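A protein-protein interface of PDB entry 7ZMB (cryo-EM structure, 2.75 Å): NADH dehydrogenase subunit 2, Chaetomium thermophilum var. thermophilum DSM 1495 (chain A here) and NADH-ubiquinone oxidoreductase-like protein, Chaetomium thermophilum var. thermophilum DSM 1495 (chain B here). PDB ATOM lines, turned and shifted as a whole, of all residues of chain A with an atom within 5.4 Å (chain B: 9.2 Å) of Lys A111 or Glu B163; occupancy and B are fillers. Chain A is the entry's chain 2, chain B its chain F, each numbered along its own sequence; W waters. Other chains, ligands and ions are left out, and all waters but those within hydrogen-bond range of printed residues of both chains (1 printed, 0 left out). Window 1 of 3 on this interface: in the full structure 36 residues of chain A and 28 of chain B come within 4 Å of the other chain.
The side-chain carboxylate (OE2) of Glu B157 is in hydrogen-bond range of the side-chain hydroxyl (OG1) of Thr A110 (2.7 Å).
OE2 of Glu B163 is in salt-bridge range of NZ of Lys A111, 3.6 Å away.
The backbone NH (N) of Glu B163 is in hydrogen-bond range of the side-chain amide oxygen (OD1) of Asn A114 (2.9 Å).
The side-chain carboxylate (OE1) of Glu B163 is in hydrogen-bond range of the side-chain hydroxyl (OH) of Tyr A392, at 2.6 Å.
The backbone carbonyl oxygen (O) of Glu B163 sits close to the side-chain amide oxygen (OD1) of Asn A408, at 3.2 Å.
OE2 of Glu B165 is in salt-bridge range of NH1 of Arg A87.
OE1 of Glu B165 lies within hydrogen-bond range of ND2 of Asn A114 (3.0 Å).
N of Glu B165 is in hydrogen-bond range of OD1 of Asn A408.
The guanidinium group (NH2) of Arg B168 is in hydrogen-bond range of the side-chain amide oxygen (OD1) of Asn A408.
The side-chain hydroxyl (OH) of Tyr A108 is in hydrogen-bond range of the guanidinium group (NH1) of Arg B184, at 3.1 Å.
The side-chain carboxylate (OE1) of Glu B121 lies within salt-bridge range of the side-chain amino group (NZ) of Lys B180.
NH2 of Arg B184 is in salt-bridge range of OE2 of Glu B121.
The guanidinium group (NH1) of Arg B184 lies within salt-bridge range of the side-chain carboxylate (OE2) of Glu B160 (3.8 Å).
The guanidinium group (NE) of Arg B168 sits at hydrogen-bond distance from the backbone carbonyl oxygen (O) of Glu B165 (2.4 Å).
NE of Arg A87 is in hydrogen-bond range of O of Ile A112 (2.9 Å).
The backbone carbonyl oxygen (O) of Lys A111 sits at hydrogen-bond distance from the side-chain hydroxyl (OH) of Tyr A392, at 2.9 Å.
CE1 of Tyr A108 touches OE2 of Glu B157, at 3.6 Å.
Lys B180 touches Tyr A108.
CE of Lys A111 touches CB of Lys B180, at 3.7 Å.
Ile B181 touches Lys A111.
Lys A111 touches Arg B184 (CE to NH1, 3.2 Å).
CD1 of Ile A112 touches CG2 of Ile B181, 3.8 Å away.
Pro B162 touches Asn A114.
NZ of Lys B173 touches CD1 of Tyr A392, at 3.7 Å.
ND2 of Asn A408 touches CB of Pro B162, at 3.4 Å.
Leu B164 touches Asn A408 (CA to OD1, 3.99 Å).
Lys A111 touches just these residues of chain B: Glu B163, Gly B177, Lys B180, Ile B181 and Arg B184.
Of the printed residues of chain B, Asn A408 touches Pro B162 (3.4 Å), Glu B163 (3.2 Å), Leu B164 (3.99 Å), Glu B165 (3.2 Å) and Arg B168 (3.0 Å).
Glu B163 touches just these residues of chain A: Lys A111, Asn A114, Tyr A392 and Asn A408.
Of the printed residues of chain A, Leu B164 touches Asn A408 (3.99 Å).
Ile B174 touches none of the printed residues of chain A.
Of the printed residues of chain A, Ile B181 touches Lys A111 and Ile A112.
Of the printed residues of chain A, Arg B184 touches Tyr A108 and Lys A111.
Of the 11 printed residues of chain A, 8 touch a printed residue of chain B.
Printed residues of chain A that touch a printed residue of chain B: Arg A87, Tyr A108, Thr A110, Lys A111, Ile A112, Asn A114, Tyr A392 and Asn A408.
Hydrophobic or aromatic side chains of chain A within 4 Å of the printed part of chain B: Tyr A108, Ile A112 and Tyr A392.
Among the printed residues, 21 pairs touch across the chains.
Among the printed residues, Asp or Glu carboxylates within 4 Å of a Lys or Arg side-chain nitrogen of the other chain: Arg A87 with Glu B165 (3.1 Å) and Lys A111 with Glu B163 (3.6 Å).
Water W1 lies within hydrogen-bond range of OE1 of Glu B160, NZ of Lys A111 and OH of Tyr A108.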
ATOM      1  N   ARG A  87      -7.732  17.414 -12.615  1.00  0.00           N
ATOM      2  CA  ARG A  87      -6.641  16.927 -11.743  1.00  0.00           C
ATOM      3  C   ARG A  87      -5.412  16.571 -12.558  1.00  0.00           C
ATOM      4  O   ARG A  87      -5.490  16.692 -13.784  1.00  0.00           O
ATOM      5  CB  ARG A  87      -7.128  15.865 -10.756  1.00  0.00           C
ATOM      6  CG  ARG A  87      -7.879  16.447  -9.571  1.00  0.00           C
ATOM      7  CD  ARG A  87      -8.631  15.358  -8.846  1.00  0.00           C
ATOM      8  NE  ARG A  87      -9.366  14.531  -9.790  1.00  0.00           N
ATOM      9  CZ  ARG A  87     -10.664  14.632 -10.032  1.00  0.00           C
ATOM     10  NH1 ARG A  87     -11.390  15.528  -9.387  1.00  0.00           N
ATOM     11  NH2 ARG A  87     -11.232  13.827 -10.908  1.00  0.00           N
ATOM     12  N   TYR A 108      -2.623   4.997 -16.039  1.00  0.00           N
ATOM     13  CA  TYR A 108      -4.079   4.982 -16.146  1.00  0.00           C
ATOM     14  C   TYR A 108      -4.616   6.303 -15.609  1.00  0.00           C
ATOM     15  O   TYR A 108      -4.709   6.502 -14.396  1.00  0.00           O
ATOM     16  CB  TYR A 108      -4.666   3.800 -15.384  1.00  0.00           C
ATOM     17  CG  TYR A 108      -6.144   3.626 -15.632  1.00  0.00           C
ATOM     18  CD1 TYR A 108      -6.663   3.711 -16.915  1.00  0.00           C
ATOM     19  CD2 TYR A 108      -7.030   3.445 -14.584  1.00  0.00           C
ATOM     20  CE1 TYR A 108      -8.010   3.576 -17.148  1.00  0.00           C
ATOM     21  CE2 TYR A 108      -8.385   3.325 -14.810  1.00  0.00           C
ATOM     22  CZ  TYR A 108      -8.867   3.395 -16.093  1.00  0.00           C
ATOM     23  OH  TYR A 108     -10.212   3.262 -16.331  1.00  0.00           O
ATOM     24  N   ARG A 109      -5.066   7.183 -16.497  1.00  0.00           N
ATOM     25  CA  ARG A 109      -5.536   8.514 -16.035  1.00  0.00           C
ATOM     26  C   ARG A 109      -7.056   8.623 -16.137  1.00  0.00           C
ATOM     27  O   ARG A 109      -7.566   9.655 -15.711  1.00  0.00           O
ATOM     28  CB  ARG A 109      -4.975   9.645 -16.898  1.00  0.00           C
ATOM     29  CG  ARG A 109      -3.817   9.295 -17.814  1.00  0.00           C
ATOM     30  CD  ARG A 109      -3.308  10.596 -18.406  1.00  0.00           C
ATOM     31  NE  ARG A 109      -1.971  10.496 -18.971  1.00  0.00           N
ATOM     32  CZ  ARG A 109      -1.199  11.531 -19.274  1.00  0.00           C
ATOM     33  NH1 ARG A 109      -1.625  12.764 -19.057  1.00  0.00           N
ATOM     34  NH2 ARG A 109       0.002  11.331 -19.781  1.00  0.00           N
ATOM     35  N   THR A 110      -7.763   7.575 -16.573  1.00  0.00           N
ATOM     36  CA  THR A 110      -9.212   7.753 -16.861  1.00  0.00           C
ATOM     37  C   THR A 110      -9.966   8.222 -15.619  1.00  0.00           C
ATOM     38  O   THR A 110     -10.769   9.163 -15.754  1.00  0.00           O
ATOM     39  CB  THR A 110      -9.843   6.540 -17.555  1.00  0.00           C
ATOM     40  OG1 THR A 110      -9.012   6.222 -18.670  1.00  0.00           O
ATOM     41  CG2 THR A 110     -11.254   6.794 -18.034  1.00  0.00           C
ATOM     42  N   LYS A 111      -9.679   7.635 -14.457  1.00  0.00           N
ATOM     43  CA  LYS A 111     -10.426   8.020 -13.237  1.00  0.00           C
ATOM     44  C   LYS A 111      -9.792   9.267 -12.610  1.00  0.00           C
ATOM     45  O   LYS A 111     -10.561  10.152 -12.222  1.00  0.00           O
ATOM     46  CB  LYS A 111     -10.507   6.822 -12.292  1.00  0.00           C
ATOM     47  CG  LYS A 111     -11.044   5.552 -12.933  1.00  0.00           C
ATOM     48  CD  LYS A 111     -11.244   4.428 -11.951  1.00  0.00           C
ATOM     49  CE  LYS A 111     -12.211   3.390 -12.469  1.00  0.00           C
ATOM     50  NZ  LYS A 111     -13.448   4.017 -12.992  1.00  0.00           N
ATOM     51  N   ILE A 112      -8.458   9.376 -12.576  1.00  0.00           N
ATOM     52  CA  ILE A 112      -7.782  10.479 -11.900  1.00  0.00           C
ATOM     53  C   ILE A 112      -8.130  11.811 -12.556  1.00  0.00           C
ATOM     54  O   ILE A 112      -8.402  12.805 -11.873  1.00  0.00           O
ATOM     55  CB  ILE A 112      -6.259  10.241 -11.881  1.00  0.00           C
ATOM     56  CG1 ILE A 112      -5.877   9.266 -10.767  1.00  0.00           C
ATOM     57  CG2 ILE A 112      -5.515  11.543 -11.694  1.00  0.00           C
ATOM     58  CD1 ILE A 112      -4.563   8.599 -10.973  1.00  0.00           C
ATOM     59  N   ILE A 113      -8.195  11.835 -13.889  1.00  0.00           N
ATOM     60  CA  ILE A 113      -8.434  13.113 -14.630  1.00  0.00           C
ATOM     61  C   ILE A 113      -9.924  13.304 -14.963  1.00  0.00           C
ATOM     62  O   ILE A 113     -10.242  14.345 -15.550  1.00  0.00           O
ATOM     63  CB  ILE A 113      -7.546  13.198 -15.886  1.00  0.00           C
ATOM     64  CG1 ILE A 113      -8.108  12.374 -17.049  1.00  0.00           C
ATOM     65  CG2 ILE A 113      -6.105  12.839 -15.557  1.00  0.00           C
ATOM     66  CD1 ILE A 113      -7.271  12.409 -18.299  1.00  0.00           C
ATOM     67  N   ASN A 114     -10.800  12.363 -14.587  1.00  0.00           N
ATOM     68  CA  ASN A 114     -12.245  12.412 -14.966  1.00  0.00           C
ATOM     69  C   ASN A 114     -12.360  12.667 -16.474  1.00  0.00           C
ATOM     70  O   ASN A 114     -13.101  13.587 -16.867  1.00  0.00           O
ATOM     71  CB  ASN A 114     -13.080  13.341 -14.089  1.00  0.00           C
ATOM     72  CG  ASN A 114     -14.562  13.035 -14.143  1.00  0.00           C
ATOM     73  OD1 ASN A 114     -14.969  12.013 -14.690  1.00  0.00           O
ATOM     74  ND2 ASN A 114     -15.374  13.910 -13.579  1.00  0.00           N
ATOM     75  N   GLY A 117     -15.932  12.858 -17.793  1.00  0.00           N
ATOM     76  CA  GLY A 117     -16.869  13.717 -17.044  1.00  0.00           C
ATOM     77  C   GLY A 117     -17.802  14.487 -17.963  1.00  0.00           C
ATOM     78  O   GLY A 117     -17.468  14.630 -19.146  1.00  0.00           O
ATOM     79  N   TYR A 392     -11.380  15.013  -4.071  1.00  0.00           N
ATOM     80  CA  TYR A 392     -11.403  13.703  -4.766  1.00  0.00           C
ATOM     81  C   TYR A 392     -10.720  12.664  -3.883  1.00  0.00           C
ATOM     82  O   TYR A 392     -11.142  11.494  -3.882  1.00  0.00           O
ATOM     83  CB  TYR A 392     -10.720  13.875  -6.122  1.00  0.00           C
ATOM     84  CG  TYR A 392     -10.625  12.650  -6.988  1.00  0.00           C
ATOM     85  CD1 TYR A 392     -11.754  12.081  -7.548  1.00  0.00           C
ATOM     86  CD2 TYR A 392      -9.395  12.083  -7.277  1.00  0.00           C
ATOM     87  CE1 TYR A 392     -11.664  10.964  -8.358  1.00  0.00           C
ATOM     88  CE2 TYR A 392      -9.289  10.967  -8.087  1.00  0.00           C
ATOM     89  CZ  TYR A 392     -10.430  10.406  -8.630  1.00  0.00           C
ATOM     90  OH  TYR A 392     -10.328   9.304  -9.425  1.00  0.00           O
ATOM     91  N   ASN A 408     -22.484  15.873  -9.090  1.00  0.00           N
ATOM     92  CA  ASN A 408     -21.462  15.923 -10.128  1.00  0.00           C
ATOM     93  C   ASN A 408     -21.412  17.277 -10.818  1.00  0.00           C
ATOM     94  O   ASN A 408     -20.337  17.721 -11.219  1.00  0.00           O
ATOM     95  CB  ASN A 408     -21.708  14.824 -11.158  1.00  0.00           C
ATOM     96  CG  ASN A 408     -20.885  13.584 -10.897  1.00  0.00           C
ATOM     97  OD1 ASN A 408     -20.046  13.559 -10.001  1.00  0.00           O
ATOM     98  ND2 ASN A 408     -21.126  12.548 -11.678  1.00  0.00           N
ATOM     99  N   GLU B 121      -9.519  -6.442 -18.292  1.00  0.00           N
ATOM    100  CA  GLU B 121     -10.590  -5.470 -18.140  1.00  0.00           C
ATOM    101  C   GLU B 121     -10.603  -4.422 -19.239  1.00  0.00           C
ATOM    102  O   GLU B 121     -11.642  -3.799 -19.465  1.00  0.00           O
ATOM    103  CB  GLU B 121     -10.488  -4.772 -16.775  1.00  0.00           C
ATOM    104  CG  GLU B 121     -11.758  -4.061 -16.334  1.00  0.00           C
ATOM    105  CD  GLU B 121     -11.735  -3.679 -14.867  1.00  0.00           C
ATOM    106  OE1 GLU B 121     -10.787  -4.079 -14.164  1.00  0.00           O
ATOM    107  OE2 GLU B 121     -12.665  -2.977 -14.419  1.00  0.00           O
ATOM    108  N   GLU B 157     -12.525   2.910 -25.400  1.00  0.00           N
ATOM    109  CA  GLU B 157     -12.550   2.700 -23.929  1.00  0.00           C
ATOM    110  C   GLU B 157     -13.985   2.442 -23.456  1.00  0.00           C
ATOM    111  O   GLU B 157     -14.911   2.934 -24.100  1.00  0.00           O
ATOM    112  CB  GLU B 157     -11.854   3.869 -23.234  1.00  0.00           C
ATOM    113  CG  GLU B 157     -11.641   3.673 -21.746  1.00  0.00           C
ATOM    114  CD  GLU B 157     -10.454   4.435 -21.189  1.00  0.00           C
ATOM    115  OE1 GLU B 157      -9.972   5.360 -21.872  1.00  0.00           O
ATOM    116  OE2 GLU B 157     -10.001   4.084 -20.084  1.00  0.00           O
ATOM    117  N   VAL B 158     -14.159   1.785 -22.310  1.00  0.00           N
ATOM    118  CA  VAL B 158     -15.535   1.595 -21.767  1.00  0.00           C
ATOM    119  C   VAL B 158     -15.925   2.853 -20.991  1.00  0.00           C
ATOM    120  O   VAL B 158     -15.090   3.361 -20.228  1.00  0.00           O
ATOM    121  CB  VAL B 158     -15.685   0.314 -20.929  1.00  0.00           C
ATOM    122  CG1 VAL B 158     -16.999   0.279 -20.164  1.00  0.00           C
ATOM    123  CG2 VAL B 158     -15.540  -0.932 -21.781  1.00  0.00           C
ATOM    124  N   ASP B 159     -17.143   3.341 -21.221  1.00  0.00           N
ATOM    125  CA  ASP B 159     -17.624   4.538 -20.503  1.00  0.00           C
ATOM    126  C   ASP B 159     -18.376   4.070 -19.255  1.00  0.00           C
ATOM    127  O   ASP B 159     -19.512   3.588 -19.387  1.00  0.00           O
ATOM    128  CB  ASP B 159     -18.404   5.445 -21.455  1.00  0.00           C
ATOM    129  CG  ASP B 159     -18.644   6.847 -20.921  1.00  0.00           C
ATOM    130  OD1 ASP B 159     -18.202   7.130 -19.793  1.00  0.00           O
ATOM    131  OD2 ASP B 159     -19.270   7.646 -21.645  1.00  0.00           O
ATOM    132  N   GLU B 160     -17.753   4.231 -18.088  1.00  0.00           N
ATOM    133  CA  GLU B 160     -18.381   3.824 -16.811  1.00  0.00           C
ATOM    134  C   GLU B 160     -19.119   5.044 -16.260  1.00  0.00           C
ATOM    135  O   GLU B 160     -19.701   4.940 -15.164  1.00  0.00           O
ATOM    136  CB  GLU B 160     -17.316   3.284 -15.857  1.00  0.00           C
ATOM    137  CG  GLU B 160     -16.667   1.996 -16.332  1.00  0.00           C
ATOM    138  CD  GLU B 160     -15.353   2.169 -17.074  1.00  0.00           C
ATOM    139  OE1 GLU B 160     -14.852   3.309 -17.126  1.00  0.00           O
ATOM    140  OE2 GLU B 160     -14.833   1.166 -17.597  1.00  0.00           O
ATOM    141  N   GLY B 161     -19.093   6.154 -17.005  1.00  0.00           N
ATOM    142  CA  GLY B 161     -19.772   7.389 -16.581  1.00  0.00           C
ATOM    143  C   GLY B 161     -18.839   8.325 -15.843  1.00  0.00           C
ATOM    144  O   GLY B 161     -17.657   7.969 -15.673  1.00  0.00           O
ATOM    145  N   PRO B 162     -19.313   9.519 -15.414  1.00  0.00           N
ATOM    146  CA  PRO B 162     -18.460  10.489 -14.750  1.00  0.00           C
ATOM    147  C   PRO B 162     -17.945  10.014 -13.389  1.00  0.00           C
ATOM    148  O   PRO B 162     -18.711   9.393 -12.676  1.00  0.00           O
ATOM    149  CB  PRO B 162     -19.400  11.678 -14.519  1.00  0.00           C
ATOM    150  CG  PRO B 162     -20.501  11.496 -15.530  1.00  0.00           C
ATOM    151  CD  PRO B 162     -20.682   9.996 -15.590  1.00  0.00           C
ATOM    152  N   GLU B 163     -16.683  10.310 -13.063  1.00  0.00           N
ATOM    153  CA  GLU B 163     -16.161   9.987 -11.746  1.00  0.00           C
ATOM    154  C   GLU B 163     -16.978  10.689 -10.674  1.00  0.00           C
ATOM    155  O   GLU B 163     -17.496  11.787 -10.877  1.00  0.00           O
ATOM    156  CB  GLU B 163     -14.694  10.390 -11.630  1.00  0.00           C
ATOM    157  CG  GLU B 163     -13.743   9.335 -12.140  1.00  0.00           C
ATOM    158  CD  GLU B 163     -13.418   8.297 -11.088  1.00  0.00           C
ATOM    159  OE1 GLU B 163     -12.805   8.654 -10.063  1.00  0.00           O
ATOM    160  OE2 GLU B 163     -13.784   7.119 -11.284  1.00  0.00           O
ATOM    161  N   LEU B 164     -17.098  10.042  -9.526  1.00  0.00           N
ATOM    162  CA  LEU B 164     -17.817  10.649  -8.418  1.00  0.00           C
ATOM    163  C   LEU B 164     -17.058  11.865  -7.908  1.00  0.00           C
ATOM    164  O   LEU B 164     -15.878  11.778  -7.562  1.00  0.00           O
ATOM    165  CB  LEU B 164     -18.020   9.631  -7.303  1.00  0.00           C
ATOM    166  CG  LEU B 164     -18.810   8.381  -7.705  1.00  0.00           C
ATOM    167  CD1 LEU B 164     -19.359   7.692  -6.486  1.00  0.00           C
ATOM    168  CD2 LEU B 164     -19.933   8.740  -8.652  1.00  0.00           C
ATOM    169  N   GLU B 165     -17.732  13.006  -7.889  1.00  0.00           N
ATOM    170  CA  GLU B 165     -17.170  14.255  -7.409  1.00  0.00           C
ATOM    171  C   GLU B 165     -18.000  14.754  -6.240  1.00  0.00           C
ATOM    172  O   GLU B 165     -19.080  14.237  -5.949  1.00  0.00           O
ATOM    173  CB  GLU B 165     -17.125  15.313  -8.516  1.00  0.00           C
ATOM    174  CG  GLU B 165     -16.546  14.826  -9.826  1.00  0.00           C
ATOM    175  CD  GLU B 165     -15.036  14.738  -9.805  1.00  0.00           C
ATOM    176  OE1 GLU B 165     -14.461  14.190 -10.766  1.00  0.00           O
ATOM    177  OE2 GLU B 165     -14.424  15.223  -8.834  1.00  0.00           O
ATOM    178  N   GLY B 166     -17.486  15.769  -5.570  1.00  0.00           N
ATOM    179  CA  GLY B 166     -18.173  16.333  -4.436  1.00  0.00           C
ATOM    180  C   GLY B 166     -17.989  15.517  -3.176  1.00  0.00           C
ATOM    181  O   GLY B 166     -17.172  14.601  -3.091  1.00  0.00           O
ATOM    182  N   ARG B 168     -18.519  12.770  -0.870  1.00  0.00           N
ATOM    183  CA  ARG B 168     -18.964  11.390  -0.954  1.00  0.00           C
ATOM    184  C   ARG B 168     -18.487  10.625   0.269  1.00  0.00           C
ATOM    185  O   ARG B 168     -17.469  10.962   0.874  1.00  0.00           O
ATOM    186  CB  ARG B 168     -18.444  10.688  -2.229  1.00  0.00           C
ATOM    187  CG  ARG B 168     -18.557  11.487  -3.499  1.00  0.00           C
ATOM    188  CD  ARG B 168     -19.989  11.574  -3.962  1.00  0.00           C
ATOM    189  NE  ARG B 168     -20.097  12.139  -5.299  1.00  0.00           N
ATOM    190  CZ  ARG B 168     -20.903  11.665  -6.241  1.00  0.00           C
ATOM    191  NH1 ARG B 168     -21.677  10.626  -5.983  1.00  0.00           N
ATOM    192  NH2 ARG B 168     -20.941  12.236  -7.433  1.00  0.00           N
ATOM    193  N   GLU B 172     -19.349   4.833  -1.115  1.00  0.00           N
ATOM    194  CA  GLU B 172     -19.721   5.249  -2.461  1.00  0.00           C
ATOM    195  C   GLU B 172     -18.499   5.335  -3.366  1.00  0.00           C
ATOM    196  O   GLU B 172     -18.546   4.917  -4.527  1.00  0.00           O
ATOM    197  CB  GLU B 172     -20.453   6.589  -2.407  1.00  0.00           C
ATOM    198  N   LYS B 173     -17.395   5.871  -2.847  1.00  0.00           N
ATOM    199  CA  LYS B 173     -16.153   5.887  -3.608  1.00  0.00           C
ATOM    200  C   LYS B 173     -15.661   4.476  -3.881  1.00  0.00           C
ATOM    201  O   LYS B 173     -15.092   4.212  -4.945  1.00  0.00           O
ATOM    202  CB  LYS B 173     -15.089   6.687  -2.857  1.00  0.00           C
ATOM    203  CG  LYS B 173     -15.427   8.155  -2.646  1.00  0.00           C
ATOM    204  CD  LYS B 173     -15.527   8.917  -3.948  1.00  0.00           C
ATOM    205  CE  LYS B 173     -14.163   9.092  -4.583  1.00  0.00           C
ATOM    206  NZ  LYS B 173     -14.225   9.903  -5.820  1.00  0.00           N
ATOM    207  N   ILE B 174     -15.861   3.559  -2.930  1.00  0.00           N
ATOM    208  CA  ILE B 174     -15.529   2.158  -3.163  1.00  0.00           C
ATOM    209  C   ILE B 174     -16.388   1.594  -4.282  1.00  0.00           C
ATOM    210  O   ILE B 174     -15.882   1.000  -5.240  1.00  0.00           O
ATOM    211  CB  ILE B 174     -15.701   1.345  -1.870  1.00  0.00           C
ATOM    212  CG1 ILE B 174     -14.738   1.835  -0.791  1.00  0.00           C
ATOM    213  CG2 ILE B 174     -15.464  -0.125  -2.136  1.00  0.00           C
ATOM    214  CD1 ILE B 174     -15.033   1.266   0.564  1.00  0.00           C
ATOM    215  N   GLU B 175     -17.706   1.789  -4.185  1.00  0.00           N
ATOM    216  CA  GLU B 175     -18.614   1.306  -5.216  1.00  0.00           C
ATOM    217  C   GLU B 175     -18.344   1.972  -6.557  1.00  0.00           C
ATOM    218  O   GLU B 175     -18.708   1.428  -7.606  1.00  0.00           O
ATOM    219  CB  GLU B 175     -20.062   1.546  -4.792  1.00  0.00           C
ATOM    220  CG  GLU B 175     -20.484   0.797  -3.541  1.00  0.00           C
ATOM    221  CD  GLU B 175     -20.750  -0.671  -3.803  1.00  0.00           C
ATOM    222  OE1 GLU B 175     -20.923  -1.043  -4.982  1.00  0.00           O
ATOM    223  OE2 GLU B 175     -20.787  -1.453  -2.829  1.00  0.00           O
ATOM    224  N   GLY B 176     -17.714   3.148  -6.547  1.00  0.00           N
ATOM    225  CA  GLY B 176     -17.425   3.831  -7.794  1.00  0.00           C
ATOM    226  C   GLY B 176     -16.450   3.069  -8.668  1.00  0.00           C
ATOM    227  O   GLY B 176     -16.570   3.069  -9.896  1.00  0.00           O
ATOM    228  N   GLY B 177     -15.480   2.403  -8.051  1.00  0.00           N
ATOM    229  CA  GLY B 177     -14.436   1.723  -8.789  1.00  0.00           C
ATOM    230  C   GLY B 177     -13.073   2.253  -8.414  1.00  0.00           C
ATOM    231  O   GLY B 177     -12.130   2.206  -9.206  1.00  0.00           O
ATOM    232  N   LEU B 178     -12.965   2.761  -7.189  1.00  0.00           N
ATOM    233  CA  LEU B 178     -11.743   3.430  -6.766  1.00  0.00           C
ATOM    234  C   LEU B 178     -10.570   2.465  -6.662  1.00  0.00           C
ATOM    235  O   LEU B 178      -9.414   2.883  -6.751  1.00  0.00           O
ATOM    236  CB  LEU B 178     -11.994   4.152  -5.445  1.00  0.00           C
ATOM    237  CG  LEU B 178     -10.849   4.922  -4.794  1.00  0.00           C
ATOM    238  CD1 LEU B 178     -10.442   6.086  -5.671  1.00  0.00           C
ATOM    239  CD2 LEU B 178     -11.314   5.436  -3.456  1.00  0.00           C
ATOM    240  N   GLU B 179     -10.830   1.176  -6.481  1.00  0.00           N
ATOM    241  CA  GLU B 179      -9.721   0.238  -6.476  1.00  0.00           C
ATOM    242  C   GLU B 179      -9.139  -0.001  -7.863  1.00  0.00           C
ATOM    243  O   GLU B 179      -8.083  -0.633  -7.966  1.00  0.00           O
ATOM    244  CB  GLU B 179     -10.162  -1.086  -5.853  1.00  0.00           C
ATOM    245  CG  GLU B 179     -10.505  -0.975  -4.378  1.00  0.00           C
ATOM    246  CD  GLU B 179     -10.329  -2.282  -3.636  1.00  0.00           C
ATOM    247  OE1 GLU B 179     -10.125  -3.320  -4.298  1.00  0.00           O
ATOM    248  OE2 GLU B 179     -10.388  -2.270  -2.388  1.00  0.00           O
ATOM    249  N   LYS B 180      -9.785   0.490  -8.925  1.00  0.00           N
ATOM    250  CA  LYS B 180      -9.319   0.248 -10.286  1.00  0.00           C
ATOM    251  C   LYS B 180      -8.204   1.180 -10.733  1.00  0.00           C
ATOM    252  O   LYS B 180      -7.562   0.891 -11.743  1.00  0.00           O
ATOM    253  CB  LYS B 180     -10.483   0.344 -11.276  1.00  0.00           C
ATOM    254  CG  LYS B 180     -11.617  -0.645 -11.063  1.00  0.00           C
ATOM    255  CD  LYS B 180     -11.216  -2.077 -11.417  1.00  0.00           C
ATOM    256  CE  LYS B 180     -10.720  -2.873 -10.209  1.00  0.00           C
ATOM    257  NZ  LYS B 180     -10.437  -4.291 -10.559  1.00  0.00           N
ATOM    258  N   ILE B 181      -7.950   2.276 -10.021  1.00  0.00           N
ATOM    259  CA  ILE B 181      -6.793   3.108 -10.341  1.00  0.00           C
ATOM    260  C   ILE B 181      -5.504   2.315 -10.213  1.00  0.00           C
ATOM    261  O   ILE B 181      -4.560   2.503 -10.990  1.00  0.00           O
ATOM    262  CB  ILE B 181      -6.775   4.383  -9.468  1.00  0.00           C
ATOM    263  CG1 ILE B 181      -8.024   5.232  -9.724  1.00  0.00           C
ATOM    264  CG2 ILE B 181      -5.488   5.180  -9.651  1.00  0.00           C
ATOM    265  CD1 ILE B 181      -9.162   4.989  -8.813  1.00  0.00           C
ATOM    266  N   PHE B 182      -5.454   1.395  -9.259  1.00  0.00           N
ATOM    267  CA  PHE B 182      -4.231   0.713  -8.887  1.00  0.00           C
ATOM    268  C   PHE B 182      -4.082  -0.642  -9.562  1.00  0.00           C
ATOM    269  O   PHE B 182      -3.127  -1.367  -9.265  1.00  0.00           O
ATOM    270  CB  PHE B 182      -4.190   0.561  -7.370  1.00  0.00           C
ATOM    271  CG  PHE B 182      -4.551   1.815  -6.637  1.00  0.00           C
ATOM    272  CD1 PHE B 182      -3.685   2.895  -6.604  1.00  0.00           C
ATOM    273  CD2 PHE B 182      -5.761   1.921  -5.996  1.00  0.00           C
ATOM    274  CE1 PHE B 182      -4.021   4.048  -5.935  1.00  0.00           C
ATOM    275  CE2 PHE B 182      -6.100   3.072  -5.325  1.00  0.00           C
ATOM    276  CZ  PHE B 182      -5.227   4.138  -5.296  1.00  0.00           C
ATOM    277  N   THR B 183      -5.005  -1.015 -10.446  1.00  0.00           N
ATOM    278  CA  THR B 183      -4.935  -2.315 -11.104  1.00  0.00           C
ATOM    279  C   THR B 183      -5.101  -2.197 -12.613  1.00  0.00           C
ATOM    280  O   THR B 183      -4.541  -2.994 -13.371  1.00  0.00           O
ATOM    281  CB  THR B 183      -6.002  -3.262 -10.553  1.00  0.00           C
ATOM    282  OG1 THR B 183      -7.303  -2.727 -10.827  1.00  0.00           O
ATOM    283  CG2 THR B 183      -5.830  -3.464  -9.055  1.00  0.00           C
ATOM    284  N   ARG B 184      -5.875  -1.215 -13.056  1.00  0.00           N
ATOM    285  CA  ARG B 184      -6.102  -1.040 -14.478  1.00  0.00           C
ATOM    286  C   ARG B 184      -4.849  -0.499 -15.156  1.00  0.00           C
ATOM    287  O   ARG B 184      -3.951   0.059 -14.521  1.00  0.00           O
ATOM    288  CB  ARG B 184      -7.298  -0.120 -14.713  1.00  0.00           C
ATOM    289  CG  ARG B 184      -8.582  -0.883 -14.900  1.00  0.00           C
ATOM    290  CD  ARG B 184      -9.750   0.003 -15.170  1.00  0.00           C
ATOM    291  NE  ARG B 184     -10.964  -0.599 -14.647  1.00  0.00           N
ATOM    292  CZ  ARG B 184     -12.120   0.037 -14.527  1.00  0.00           C
ATOM    293  NH1 ARG B 184     -12.220   1.304 -14.899  1.00  0.00           N
ATOM    294  NH2 ARG B 184     -13.180  -0.593 -14.040  1.00  0.00           N
HETATM  295  O   HOH W   1     -13.000   4.931 -15.878  1.00  0.00           O
